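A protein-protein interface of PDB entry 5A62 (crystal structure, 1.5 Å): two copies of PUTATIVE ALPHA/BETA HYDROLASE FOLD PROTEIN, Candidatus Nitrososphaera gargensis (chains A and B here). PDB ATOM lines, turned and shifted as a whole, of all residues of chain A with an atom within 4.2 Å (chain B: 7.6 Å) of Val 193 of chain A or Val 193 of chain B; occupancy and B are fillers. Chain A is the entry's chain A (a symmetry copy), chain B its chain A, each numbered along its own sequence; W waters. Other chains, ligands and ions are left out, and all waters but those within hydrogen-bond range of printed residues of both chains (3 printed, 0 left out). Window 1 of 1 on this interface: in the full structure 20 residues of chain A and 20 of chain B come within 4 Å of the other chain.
Water W3 lies within hydrogen-bond range of the side-chain carboxylate (OD2) of Asp 76 of chain B (2.8 Å), the guanidinium group (NE) of Arg 141 of chain A (2.9 Å) and the side-chain hydroxyl (OG1) of Thr 73 of chain B (3.0 Å). Water W2 lies within hydrogen-bond range of NE of Arg 141 of chain B (2.9 Å) and OG1 of Thr 73 of chain A (3.0 Å). Water W1 bridges O of Tyr 196 of chain B and O of Tyr 196 of chain A.
Tyr 72 of chain A touches Val 193 of chain B, and with the chains exchanged Val 193 of chain A touches Tyr 72 of chain B. Thr 73 of chain A touches Arg 141 of chain B, and with the chains exchanged Arg 141 of chain A touches Thr 73 of chain B. Val 193 of chain B touches its own counterpart, Val 193 of chain A. Tyr 196 of chain A touches its own counterpart, Tyr 196 of chain B. Of the 9 pairs that touch across the chains among the printed residues, 6 have their exchanged pair printed and touching as well.
Hydrophobic or aromatic side chains of chain A within 4 Å of the printed part of chain B: Val 189, Val 193 and Tyr 196. Of the 22 printed residues of chain B, 7 touch a printed residue of chain A. Printed residues of chain B that touch a printed residue of chain A: Ala 71, Tyr 72, Thr 73, Arg 141, Val 193, Tyr 196 and Thr 197. Hydrophobic or aromatic side chains of chain B within 4 Å of the printed part of chain A: Ala 71, Val 193 and Tyr 196. Among the printed residues, 9 pairs touch across the chains.
Of the printed residues of chain B, Tyr 72 of chain A touches Val 193. Of the printed residues of chain B, Ala 190 of chain A touches Ala 71 (3.7 Å). Of the printed residues of chain A, Arg 141 of chain B touches Thr 73. Phe 188 of chain B touches none of the printed residues of chain A. Of chain A, only Tyr 72 and Val 193 come within 4 Å of Val 193 of chain B. Printed residues of chain A within 4 Å of Tyr 196 of chain B: Tyr 196 (3.7 Å). The nearest residue of chain B that does not touch Val 193 of chain A is Thr 73 of chain B (4.1 Å). The nearest residue of chain A that does not touch Val 193 of chain B is Thr 73 of chain A (4.1 Å). The nearest printed residue of chain B that does not touch Arg 141 of chain A is Asp 76 of chain B (4.9 Å).
Among the printed residues, merely in contact across the chains: Tyr 72 of chain A with Val 193 of chain B, Thr 73 of chain A with Arg 141 of chain B, Arg 141 of chain A with Thr 73 of chain B, Val 189 of chain A with Ala 71 of chain B, Ala 190 of chain A with Ala 71 of chain B, Val 193 of chain A with Tyr 72 of chain B, Val 193 of chain A with Val 193 of chain B, Tyr 196 of chain A with Tyr 196 of chain B and Tyr 196 of chain A with Thr 197 of chain B.
N of Thr 73 of chain B sits at hydrogen-bond distance from OD2 of Asp 76 of chain B. The backbone NH (N) of Met 74 of chain B sits at hydrogen-bond distance from the side-chain hydroxyl (OG1) of Thr 197 of chain B, 2.8 Å away. NH1 of Arg 141 of chain B sits at hydrogen-bond distance from OG1 of Thr 192 of chain B, at 2.9 Å. O of Ala 194 of chain B lies within hydrogen-bond range of OG1 of Thr 197 of chain B. The guanidinium group of Arg 141 of chain A is in hydrogen-bond range of the side-chain hydroxyl of Thr 192 of chain A, at 2.9 Å. The backbone carbonyl oxygen (O) of Val 189 of chain A sits at hydrogen-bond distance from the side-chain hydroxyl (OG1) of Thr 192 of chain A, at 3.0 Å.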
ATOM      1  N   TYR A  72      13.219  18.892 -25.970  1.00  0.00           N
ATOM      2  CA  TYR A  72      14.171  19.292 -27.013  1.00  0.00           C
ATOM      3  C   TYR A  72      13.427  19.606 -28.264  1.00  0.00           C
ATOM      4  O   TYR A  72      12.204  19.365 -28.372  1.00  0.00           O
ATOM      5  CB  TYR A  72      15.170  18.183 -27.261  1.00  0.00           C
ATOM      6  CG  TYR A  72      14.589  16.839 -27.622  1.00  0.00           C
ATOM      7  CD1 TYR A  72      14.062  16.626 -28.879  1.00  0.00           C
ATOM      8  CD2 TYR A  72      14.379  15.845 -26.674  1.00  0.00           C
ATOM      9  CE1 TYR A  72      13.466  15.460 -29.216  1.00  0.00           C
ATOM     10  CE2 TYR A  72      13.792  14.625 -27.009  1.00  0.00           C
ATOM     11  CZ  TYR A  72      13.324  14.440 -28.303  1.00  0.00           C
ATOM     12  OH  TYR A  72      12.740  13.259 -28.679  1.00  0.00           O
ATOM     13  N   THR A  73      14.107  20.148 -29.242  1.00  0.00           N
ATOM     14  CA  THR A  73      13.541  20.441 -30.565  1.00  0.00           C
ATOM     15  C   THR A  73      14.078  19.429 -31.534  1.00  0.00           C
ATOM     16  O   THR A  73      15.062  18.695 -31.291  1.00  0.00           O
ATOM     17  CB  THR A  73      13.890  21.816 -31.073  1.00  0.00           C
ATOM     18  OG1 THR A  73      15.323  21.898 -31.285  1.00  0.00           O
ATOM     19  CG2 THR A  73      13.453  22.871 -30.084  1.00  0.00           C
ATOM     20  N   ARG A 141       0.024  10.618 -24.764  1.00  0.00           N
ATOM     21  CA  ARG A 141       0.847  11.151 -23.679  1.00  0.00           C
ATOM     22  C   ARG A 141       0.184  10.927 -22.309  1.00  0.00           C
ATOM     23  O   ARG A 141       0.845  10.550 -21.350  1.00  0.00           O
ATOM     24  CB  ARG A 141       1.173  12.645 -23.862  1.00  0.00           C
ATOM     25  CG  ARG A 141       2.266  12.912 -24.896  1.00  0.00           C
ATOM     26  CD  ARG A 141       2.707  14.375 -24.882  1.00  0.00           C
ATOM     27  NE  ARG A 141       1.695  15.261 -25.353  1.00  0.00           N
ATOM     28  CZ  ARG A 141       1.474  15.542 -26.618  1.00  0.00           C
ATOM     29  NH1 ARG A 141       2.279  15.009 -27.514  1.00  0.00           N
ATOM     30  NH2 ARG A 141       0.472  16.308 -26.976  1.00  0.00           N
ATOM     31  N   VAL A 189       7.064  11.129 -24.355  1.00  0.00           N
ATOM     32  CA  VAL A 189       6.498  12.445 -24.219  1.00  0.00           C
ATOM     33  C   VAL A 189       7.323  13.474 -24.958  1.00  0.00           C
ATOM     34  O   VAL A 189       6.801  14.244 -25.767  1.00  0.00           O
ATOM     35  CB  VAL A 189       6.266  12.799 -22.773  1.00  0.00           C
ATOM     36  CG1 VAL A 189       5.838  14.227 -22.628  1.00  0.00           C
ATOM     37  CG2 VAL A 189       5.193  11.870 -22.193  1.00  0.00           C
ATOM     38  N   ALA A 190       8.629  13.501 -24.746  1.00  0.00           N
ATOM     39  CA  ALA A 190       9.460  14.495 -25.366  1.00  0.00           C
ATOM     40  C   ALA A 190       9.455  14.370 -26.875  1.00  0.00           C
ATOM     41  O   ALA A 190       9.491  15.379 -27.582  1.00  0.00           O
ATOM     42  CB  ALA A 190      10.846  14.398 -24.893  1.00  0.00           C
ATOM     43  N   ALA A 191       9.459  13.186 -27.421  1.00  0.00           N
ATOM     44  CA  ALA A 191       9.533  13.002 -28.857  1.00  0.00           C
ATOM     45  C   ALA A 191       8.262  13.520 -29.517  1.00  0.00           C
ATOM     46  O   ALA A 191       8.295  14.170 -30.559  1.00  0.00           O
ATOM     47  CB  ALA A 191       9.840  11.587 -29.210  1.00  0.00           C
ATOM     48  N   THR A 192       7.142  13.162 -28.913  1.00  0.00           N
ATOM     49  CA  THR A 192       5.891  13.624 -29.462  1.00  0.00           C
ATOM     50  C   THR A 192       5.760  15.169 -29.420  1.00  0.00           C
ATOM     51  O   THR A 192       5.263  15.836 -30.326  1.00  0.00           O
ATOM     52  CB  THR A 192       4.676  12.937 -28.879  1.00  0.00           C
ATOM     53  OG1 THR A 192       4.553  13.255 -27.500  1.00  0.00           O
ATOM     54  CG2 THR A 192       4.670  11.463 -29.108  1.00  0.00           C
ATOM     55  N   VAL A 193       6.207  15.766 -28.324  1.00  0.00           N
ATOM     56  CA  VAL A 193       6.215  17.221 -28.215  1.00  0.00           C
ATOM     57  C   VAL A 193       7.145  17.819 -29.322  1.00  0.00           C
ATOM     58  O   VAL A 193       6.853  18.843 -29.913  1.00  0.00           O
ATOM     59  CB  VAL A 193       6.602  17.655 -26.796  1.00  0.00           C
ATOM     60  CG1 VAL A 193       6.920  19.141 -26.757  1.00  0.00           C
ATOM     61  CG2 VAL A 193       5.509  17.275 -25.813  1.00  0.00           C
ATOM     62  N   ALA A 194       8.302  17.192 -29.535  1.00  0.00           N
ATOM     63  CA  ALA A 194       9.261  17.681 -30.505  1.00  0.00           C
ATOM     64  C   ALA A 194       8.674  17.783 -31.893  1.00  0.00           C
ATOM     65  O   ALA A 194       9.170  18.546 -32.727  1.00  0.00           O
ATOM     66  CB  ALA A 194      10.517  16.866 -30.508  1.00  0.00           C
ATOM     67  N   LEU A 195       7.668  16.983 -32.186  1.00  0.00           N
ATOM     68  CA  LEU A 195       7.070  17.067 -33.531  1.00  0.00           C
ATOM     69  C   LEU A 195       6.552  18.445 -33.833  1.00  0.00           C
ATOM     70  O   LEU A 195       6.469  18.823 -34.999  1.00  0.00           O
ATOM     71  CB  LEU A 195       5.943  16.023 -33.687  1.00  0.00           C
ATOM     72  CG  LEU A 195       6.427  14.566 -33.540  1.00  0.00           C
ATOM     73  CD1 LEU A 195       5.234  13.668 -33.625  1.00  0.00           C
ATOM     74  CD2 LEU A 195       7.474  14.211 -34.558  1.00  0.00           C
ATOM     75  N   TYR A 196       6.137  19.196 -32.851  1.00  0.00           N
ATOM     76  CA  TYR A 196       5.686  20.590 -33.083  1.00  0.00           C
ATOM     77  C   TYR A 196       6.765  21.546 -33.497  1.00  0.00           C
ATOM     78  O   TYR A 196       6.519  22.664 -33.938  1.00  0.00           O
ATOM     79  CB  TYR A 196       5.046  21.160 -31.813  1.00  0.00           C
ATOM     80  CG  TYR A 196       3.698  20.583 -31.474  1.00  0.00           C
ATOM     81  CD1 TYR A 196       2.560  21.179 -31.980  1.00  0.00           C
ATOM     82  CD2 TYR A 196       3.524  19.526 -30.615  1.00  0.00           C
ATOM     83  CE1 TYR A 196       1.318  20.670 -31.703  1.00  0.00           C
ATOM     84  CE2 TYR A 196       2.267  19.072 -30.303  1.00  0.00           C
ATOM     85  CZ  TYR A 196       1.172  19.647 -30.863  1.00  0.00           C
ATOM     86  OH  TYR A 196      -0.100  19.154 -30.540  1.00  0.00           O
ATOM     87  N   ILE B  32       8.221  32.978 -18.676  1.00  0.00           N
ATOM     88  CA  ILE B  32       9.348  32.064 -18.692  1.00  0.00           C
ATOM     89  C   ILE B  32      10.529  32.717 -18.000  1.00  0.00           C
ATOM     90  O   ILE B  32      10.857  33.872 -18.334  1.00  0.00           O
ATOM     91  CB  ILE B  32       9.718  31.627 -20.126  1.00  0.00           C
ATOM     92  CG1 ILE B  32       8.565  30.809 -20.725  1.00  0.00           C
ATOM     93  CG2 ILE B  32      11.021  30.843 -20.123  1.00  0.00           C
ATOM     94  CD1 ILE B  32       8.813  30.388 -22.165  1.00  0.00           C
ATOM     95  N   GLY B  70       9.795  15.661 -18.576  1.00  0.00           N
ATOM     96  CA  GLY B  70      10.488  16.873 -18.705  1.00  0.00           C
ATOM     97  C   GLY B  70      10.119  17.722 -19.922  1.00  0.00           C
ATOM     98  O   GLY B  70      10.828  18.676 -20.262  1.00  0.00           O
ATOM     99  N   ALA B  71       9.018  17.355 -20.547  1.00  0.00           N
ATOM    100  CA  ALA B  71       8.450  18.041 -21.712  1.00  0.00           C
ATOM    101  C   ALA B  71       6.989  18.057 -21.545  1.00  0.00           C
ATOM    102  O   ALA B  71       6.428  17.130 -20.951  1.00  0.00           O
ATOM    103  CB  ALA B  71       8.792  17.339 -23.028  1.00  0.00           C
ATOM    104  N   TYR B  72       6.342  19.035 -22.166  1.00  0.00           N
ATOM    105  CA  TYR B  72       4.882  19.145 -22.061  1.00  0.00           C
ATOM    106  C   TYR B  72       4.382  20.080 -23.107  1.00  0.00           C
ATOM    107  O   TYR B  72       5.169  20.759 -23.803  1.00  0.00           O
ATOM    108  CB  TYR B  72       4.494  19.641 -20.685  1.00  0.00           C
ATOM    109  CG  TYR B  72       5.113  20.947 -20.254  1.00  0.00           C
ATOM    110  CD1 TYR B  72       4.667  22.136 -20.793  1.00  0.00           C
ATOM    111  CD2 TYR B  72       6.260  20.999 -19.472  1.00  0.00           C
ATOM    112  CE1 TYR B  72       5.246  23.320 -20.488  1.00  0.00           C
ATOM    113  CE2 TYR B  72       6.854  22.212 -19.124  1.00  0.00           C
ATOM    114  CZ  TYR B  72       6.336  23.388 -19.651  1.00  0.00           C
ATOM    115  OH  TYR B  72       6.886  24.603 -19.337  1.00  0.00           O
ATOM    116  N   THR B  73       3.085  20.157 -23.266  1.00  0.00           N
ATOM    117  CA  THR B  73       2.432  21.089 -24.195  1.00  0.00           C
ATOM    118  C   THR B  73       1.808  22.187 -23.386  1.00  0.00           C
ATOM    119  O   THR B  73       1.625  22.117 -22.150  1.00  0.00           O
ATOM    120  CB  THR B  73       1.356  20.443 -25.029  1.00  0.00           C
ATOM    121  OG1 THR B  73       0.277  20.005 -24.163  1.00  0.00           O
ATOM    122  CG2 THR B  73       1.914  19.266 -25.794  1.00  0.00           C
ATOM    123  N   MET B  74       1.408  23.259 -24.059  1.00  0.00           N
ATOM    124  CA  MET B  74       0.661  24.289 -23.385  1.00  0.00           C
ATOM    125  C   MET B  74      -0.563  23.749 -22.686  1.00  0.00           C
ATOM    126  O   MET B  74      -0.900  24.216 -21.590  1.00  0.00           O
ATOM    127  CB  MET B  74       0.208  25.386 -24.359  1.00  0.00           C
ATOM    128  CG  MET B  74       1.266  26.301 -24.947  1.00  0.00           C
ATOM    129  SD  MET B  74       2.407  27.018 -23.761  1.00  0.00           S
ATOM    130  CE  MET B  74       1.270  27.941 -22.840  1.00  0.00           C
ATOM    131  N   ASP B  76      -0.927  21.107 -21.058  1.00  0.00           N
ATOM    132  CA  ASP B  76      -0.514  20.631 -19.762  1.00  0.00           C
ATOM    133  C   ASP B  76      -0.429  21.760 -18.752  1.00  0.00           C
ATOM    134  O   ASP B  76      -0.795  21.575 -17.611  1.00  0.00           O
ATOM    135  CB  ASP B  76       0.782  19.861 -19.860  1.00  0.00           C
ATOM    136  CG  ASP B  76       0.614  18.597 -20.649  1.00  0.00           C
ATOM    137  OD1 ASP B  76      -0.259  17.759 -20.278  1.00  0.00           O
ATOM    138  OD2 ASP B  76       1.377  18.372 -21.624  1.00  0.00           O
ATOM    139  N   LEU B 134      10.607  32.671 -32.534  1.00  0.00           N
ATOM    140  CA  LEU B 134      11.186  31.717 -31.580  1.00  0.00           C
ATOM    141  C   LEU B 134      12.635  31.335 -31.900  1.00  0.00           C
ATOM    142  O   LEU B 134      13.267  30.607 -31.162  1.00  0.00           O
ATOM    143  CB  LEU B 134      10.331  30.453 -31.533  1.00  0.00           C
ATOM    144  CG  LEU B 134       8.900  30.665 -31.096  1.00  0.00           C
ATOM    145  CD1 LEU B 134       8.169  29.370 -30.963  1.00  0.00           C
ATOM    146  CD2 LEU B 134       8.813  31.431 -29.806  1.00  0.00           C
ATOM    147  N   HIS B 137      15.418  31.441 -29.187  1.00  0.00           N
ATOM    148  CA  HIS B 137      15.493  30.494 -28.088  1.00  0.00           C
ATOM    149  C   HIS B 137      16.369  29.306 -28.356  1.00  0.00           C
ATOM    150  O   HIS B 137      16.717  28.567 -27.445  1.00  0.00           O
ATOM    151  CB  HIS B 137      14.077  30.010 -27.710  1.00  0.00           C
ATOM    152  CG  HIS B 137      13.140  31.075 -27.258  1.00  0.00           C
ATOM    153  ND1 HIS B 137      11.789  31.018 -27.495  1.00  0.00           N
ATOM    154  CD2 HIS B 137      13.333  32.147 -26.477  1.00  0.00           C
ATOM    155  CE1 HIS B 137      11.210  32.102 -27.013  1.00  0.00           C
ATOM    156  NE2 HIS B 137      12.122  32.783 -26.351  1.00  0.00           N
ATOM    157  N   ARG B 141      18.554  28.296 -25.188  1.00  0.00           N
ATOM    158  CA  ARG B 141      18.577  26.914 -24.711  1.00  0.00           C
ATOM    159  C   ARG B 141      20.012  26.363 -24.655  1.00  0.00           C
ATOM    160  O   ARG B 141      20.389  25.698 -23.699  1.00  0.00           O
ATOM    161  CB  ARG B 141      17.692  25.980 -25.558  1.00  0.00           C
ATOM    162  CG  ARG B 141      16.199  26.115 -25.263  1.00  0.00           C
ATOM    163  CD  ARG B 141      15.388  25.024 -25.961  1.00  0.00           C
ATOM    164  NE  ARG B 141      15.377  25.165 -27.378  1.00  0.00           N
ATOM    165  CZ  ARG B 141      14.549  25.936 -28.048  1.00  0.00           C
ATOM    166  NH1 ARG B 141      13.629  26.585 -27.367  1.00  0.00           N
ATOM    167  NH2 ARG B 141      14.653  26.072 -29.348  1.00  0.00           N
ATOM    168  N   GLY B 187      13.460  23.302 -16.726  1.00  0.00           N
ATOM    169  CA  GLY B 187      12.264  24.083 -16.810  1.00  0.00           C
ATOM    170  C   GLY B 187      12.333  25.143 -17.866  1.00  0.00           C
ATOM    171  O   GLY B 187      11.306  25.410 -18.541  1.00  0.00           O
ATOM    172  N   PHE B 188      13.441  25.855 -18.013  1.00  0.00           N
ATOM    173  CA  PHE B 188      13.592  26.828 -19.064  1.00  0.00           C
ATOM    174  C   PHE B 188      13.450  26.163 -20.421  1.00  0.00           C
ATOM    175  O   PHE B 188      12.728  26.677 -21.289  1.00  0.00           O
ATOM    176  CB  PHE B 188      14.977  27.495 -18.919  1.00  0.00           C
ATOM    177  CG  PHE B 188      15.188  28.543 -19.977  1.00  0.00           C
ATOM    178  CD1 PHE B 188      14.644  29.807 -19.864  1.00  0.00           C
ATOM    179  CD2 PHE B 188      15.954  28.270 -21.097  1.00  0.00           C
ATOM    180  CE1 PHE B 188      14.822  30.742 -20.881  1.00  0.00           C
ATOM    181  CE2 PHE B 188      16.122  29.195 -22.089  1.00  0.00           C
ATOM    182  CZ  PHE B 188      15.541  30.377 -21.991  1.00  0.00           C
ATOM    183  N   VAL B 189      14.203  25.085 -20.632  1.00  0.00           N
ATOM    184  CA  VAL B 189      14.165  24.375 -21.884  1.00  0.00           C
ATOM    185  C   VAL B 189      12.759  23.930 -22.217  1.00  0.00           C
ATOM    186  O   VAL B 189      12.252  24.194 -23.309  1.00  0.00           O
ATOM    187  CB  VAL B 189      15.166  23.250 -21.911  1.00  0.00           C
ATOM    188  CG1 VAL B 189      15.005  22.413 -23.142  1.00  0.00           C
ATOM    189  CG2 VAL B 189      16.582  23.834 -21.857  1.00  0.00           C
ATOM    190  N   ALA B 190      12.070  23.284 -21.290  1.00  0.00           N
ATOM    191  CA  ALA B 190      10.754  22.776 -21.564  1.00  0.00           C
ATOM    192  C   ALA B 190       9.776  23.889 -21.872  1.00  0.00           C
ATOM    193  O   ALA B 190       8.897  23.726 -22.720  1.00  0.00           O
ATOM    194  CB  ALA B 190      10.239  21.999 -20.430  1.00  0.00           C
ATOM    195  N   ALA B 191       9.839  25.004 -21.199  1.00  0.00           N
ATOM    196  CA  ALA B 191       8.882  26.075 -21.394  1.00  0.00           C
ATOM    197  C   ALA B 191       9.042  26.673 -22.786  1.00  0.00           C
ATOM    198  O   ALA B 191       8.070  26.966 -23.477  1.00  0.00           O
ATOM    199  CB  ALA B 191       8.973  27.092 -20.308  1.00  0.00           C
ATOM    200  N   THR B 192      10.292  26.900 -23.148  1.00  0.00           N
ATOM    201  CA  THR B 192      10.536  27.449 -24.459  1.00  0.00           C
ATOM    202  C   THR B 192      10.074  26.499 -25.595  1.00  0.00           C
ATOM    203  O   THR B 192       9.523  26.885 -26.625  1.00  0.00           O
ATOM    204  CB  THR B 192      11.955  27.933 -24.667  1.00  0.00           C
ATOM    205  OG1 THR B 192      12.854  26.834 -24.612  1.00  0.00           O
ATOM    206  CG2 THR B 192      12.349  29.016 -23.721  1.00  0.00           C
ATOM    207  N   VAL B 193      10.318  25.209 -25.415  1.00  0.00           N
ATOM    208  CA  VAL B 193       9.848  24.218 -26.378  1.00  0.00           C
ATOM    209  C   VAL B 193       8.285  24.255 -26.439  1.00  0.00           C
ATOM    210  O   VAL B 193       7.687  24.125 -27.492  1.00  0.00           O
ATOM    211  CB  VAL B 193      10.411  22.830 -26.044  1.00  0.00           C
ATOM    212  CG1 VAL B 193       9.685  21.753 -26.835  1.00  0.00           C
ATOM    213  CG2 VAL B 193      11.911  22.801 -26.275  1.00  0.00           C
ATOM    214  N   ALA B 194       7.643  24.365 -25.276  1.00  0.00           N
ATOM    215  CA  ALA B 194       6.195  24.367 -25.208  1.00  0.00           C
ATOM    216  C   ALA B 194       5.581  25.471 -26.036  1.00  0.00           C
ATOM    217  O   ALA B 194       4.418  25.378 -26.436  1.00  0.00           O
ATOM    218  CB  ALA B 194       5.703  24.415 -23.795  1.00  0.00           C
ATOM    219  N   LEU B 195       6.313  26.546 -26.251  1.00  0.00           N
ATOM    220  CA  LEU B 195       5.742  27.636 -27.063  1.00  0.00           C
ATOM    221  C   LEU B 195       5.352  27.169 -28.437  1.00  0.00           C
ATOM    222  O   LEU B 195       4.470  27.761 -29.055  1.00  0.00           O
ATOM    223  CB  LEU B 195       6.734  28.816 -27.157  1.00  0.00           C
ATOM    224  CG  LEU B 195       7.069  29.450 -25.792  1.00  0.00           C
ATOM    225  CD1 LEU B 195       8.096  30.514 -26.013  1.00  0.00           C
ATOM    226  CD2 LEU B 195       5.846  29.982 -25.099  1.00  0.00           C
ATOM    227  N   TYR B 196       6.004  26.180 -28.981  1.00  0.00           N
ATOM    228  CA  TYR B 196       5.614  25.631 -30.302  1.00  0.00           C
ATOM    229  C   TYR B 196       4.296  24.913 -30.328  1.00  0.00           C
ATOM    230  O   TYR B 196       3.737  24.605 -31.375  1.00  0.00           O
ATOM    231  CB  TYR B 196       6.672  24.641 -30.801  1.00  0.00           C
ATOM    232  CG  TYR B 196       7.968  25.271 -31.237  1.00  0.00           C
ATOM    233  CD1 TYR B 196       8.119  25.665 -32.552  1.00  0.00           C
ATOM    234  CD2 TYR B 196       9.055  25.411 -30.410  1.00  0.00           C
ATOM    235  CE1 TYR B 196       9.280  26.255 -32.979  1.00  0.00           C
ATOM    236  CE2 TYR B 196      10.228  25.948 -30.876  1.00  0.00           C
ATOM    237  CZ  TYR B 196      10.324  26.377 -32.161  1.00  0.00           C
ATOM    238  OH  TYR B 196      11.529  26.937 -32.607  1.00  0.00           O
ATOM    239  N   THR B 197       3.767  24.601 -29.138  1.00  0.00           N
ATOM    240  CA  THR B 197       2.556  23.789 -29.004  1.00  0.00           C
ATOM    241  C   THR B 197       1.330  24.626 -28.771  1.00  0.00           C
ATOM    242  O   THR B 197       0.237  24.057 -28.541  1.00  0.00           O
ATOM    243  CB  THR B 197       2.682  22.736 -27.887  1.00  0.00           C
ATOM    244  OG1 THR B 197       2.629  23.403 -26.622  1.00  0.00           O
ATOM    245  CG2 THR B 197       3.961  22.008 -27.993  1.00  0.00           C
ATOM    246  N   ILE B 198       1.431  25.958 -28.877  1.00  0.00           N
ATOM    247  CA  ILE B 198       0.227  26.823 -28.727  1.00  0.00           C
ATOM    248  C   ILE B 198      -0.707  26.517 -29.920  1.00  0.00           C
ATOM    249  O   ILE B 198      -0.205  26.534 -31.058  1.00  0.00           O
ATOM    250  CB  ILE B 198       0.625  28.263 -28.797  1.00  0.00           C
ATOM    251  CG1 ILE B 198       1.536  28.649 -27.621  1.00  0.00           C
ATOM    252  CG2 ILE B 198      -0.592  29.148 -28.851  1.00  0.00           C
ATOM    253  CD1 ILE B 198       2.230  29.983 -27.859  1.00  0.00           C
HETATM  254  O   HOH W   1       4.195  24.571 -34.379  1.00  0.00           O
HETATM  255  O   HOH W   2      16.829  23.555 -29.262  1.00  0.00           O
HETATM  256  O   HOH W   3       0.092  17.022 -23.748  1.00  0.00           O
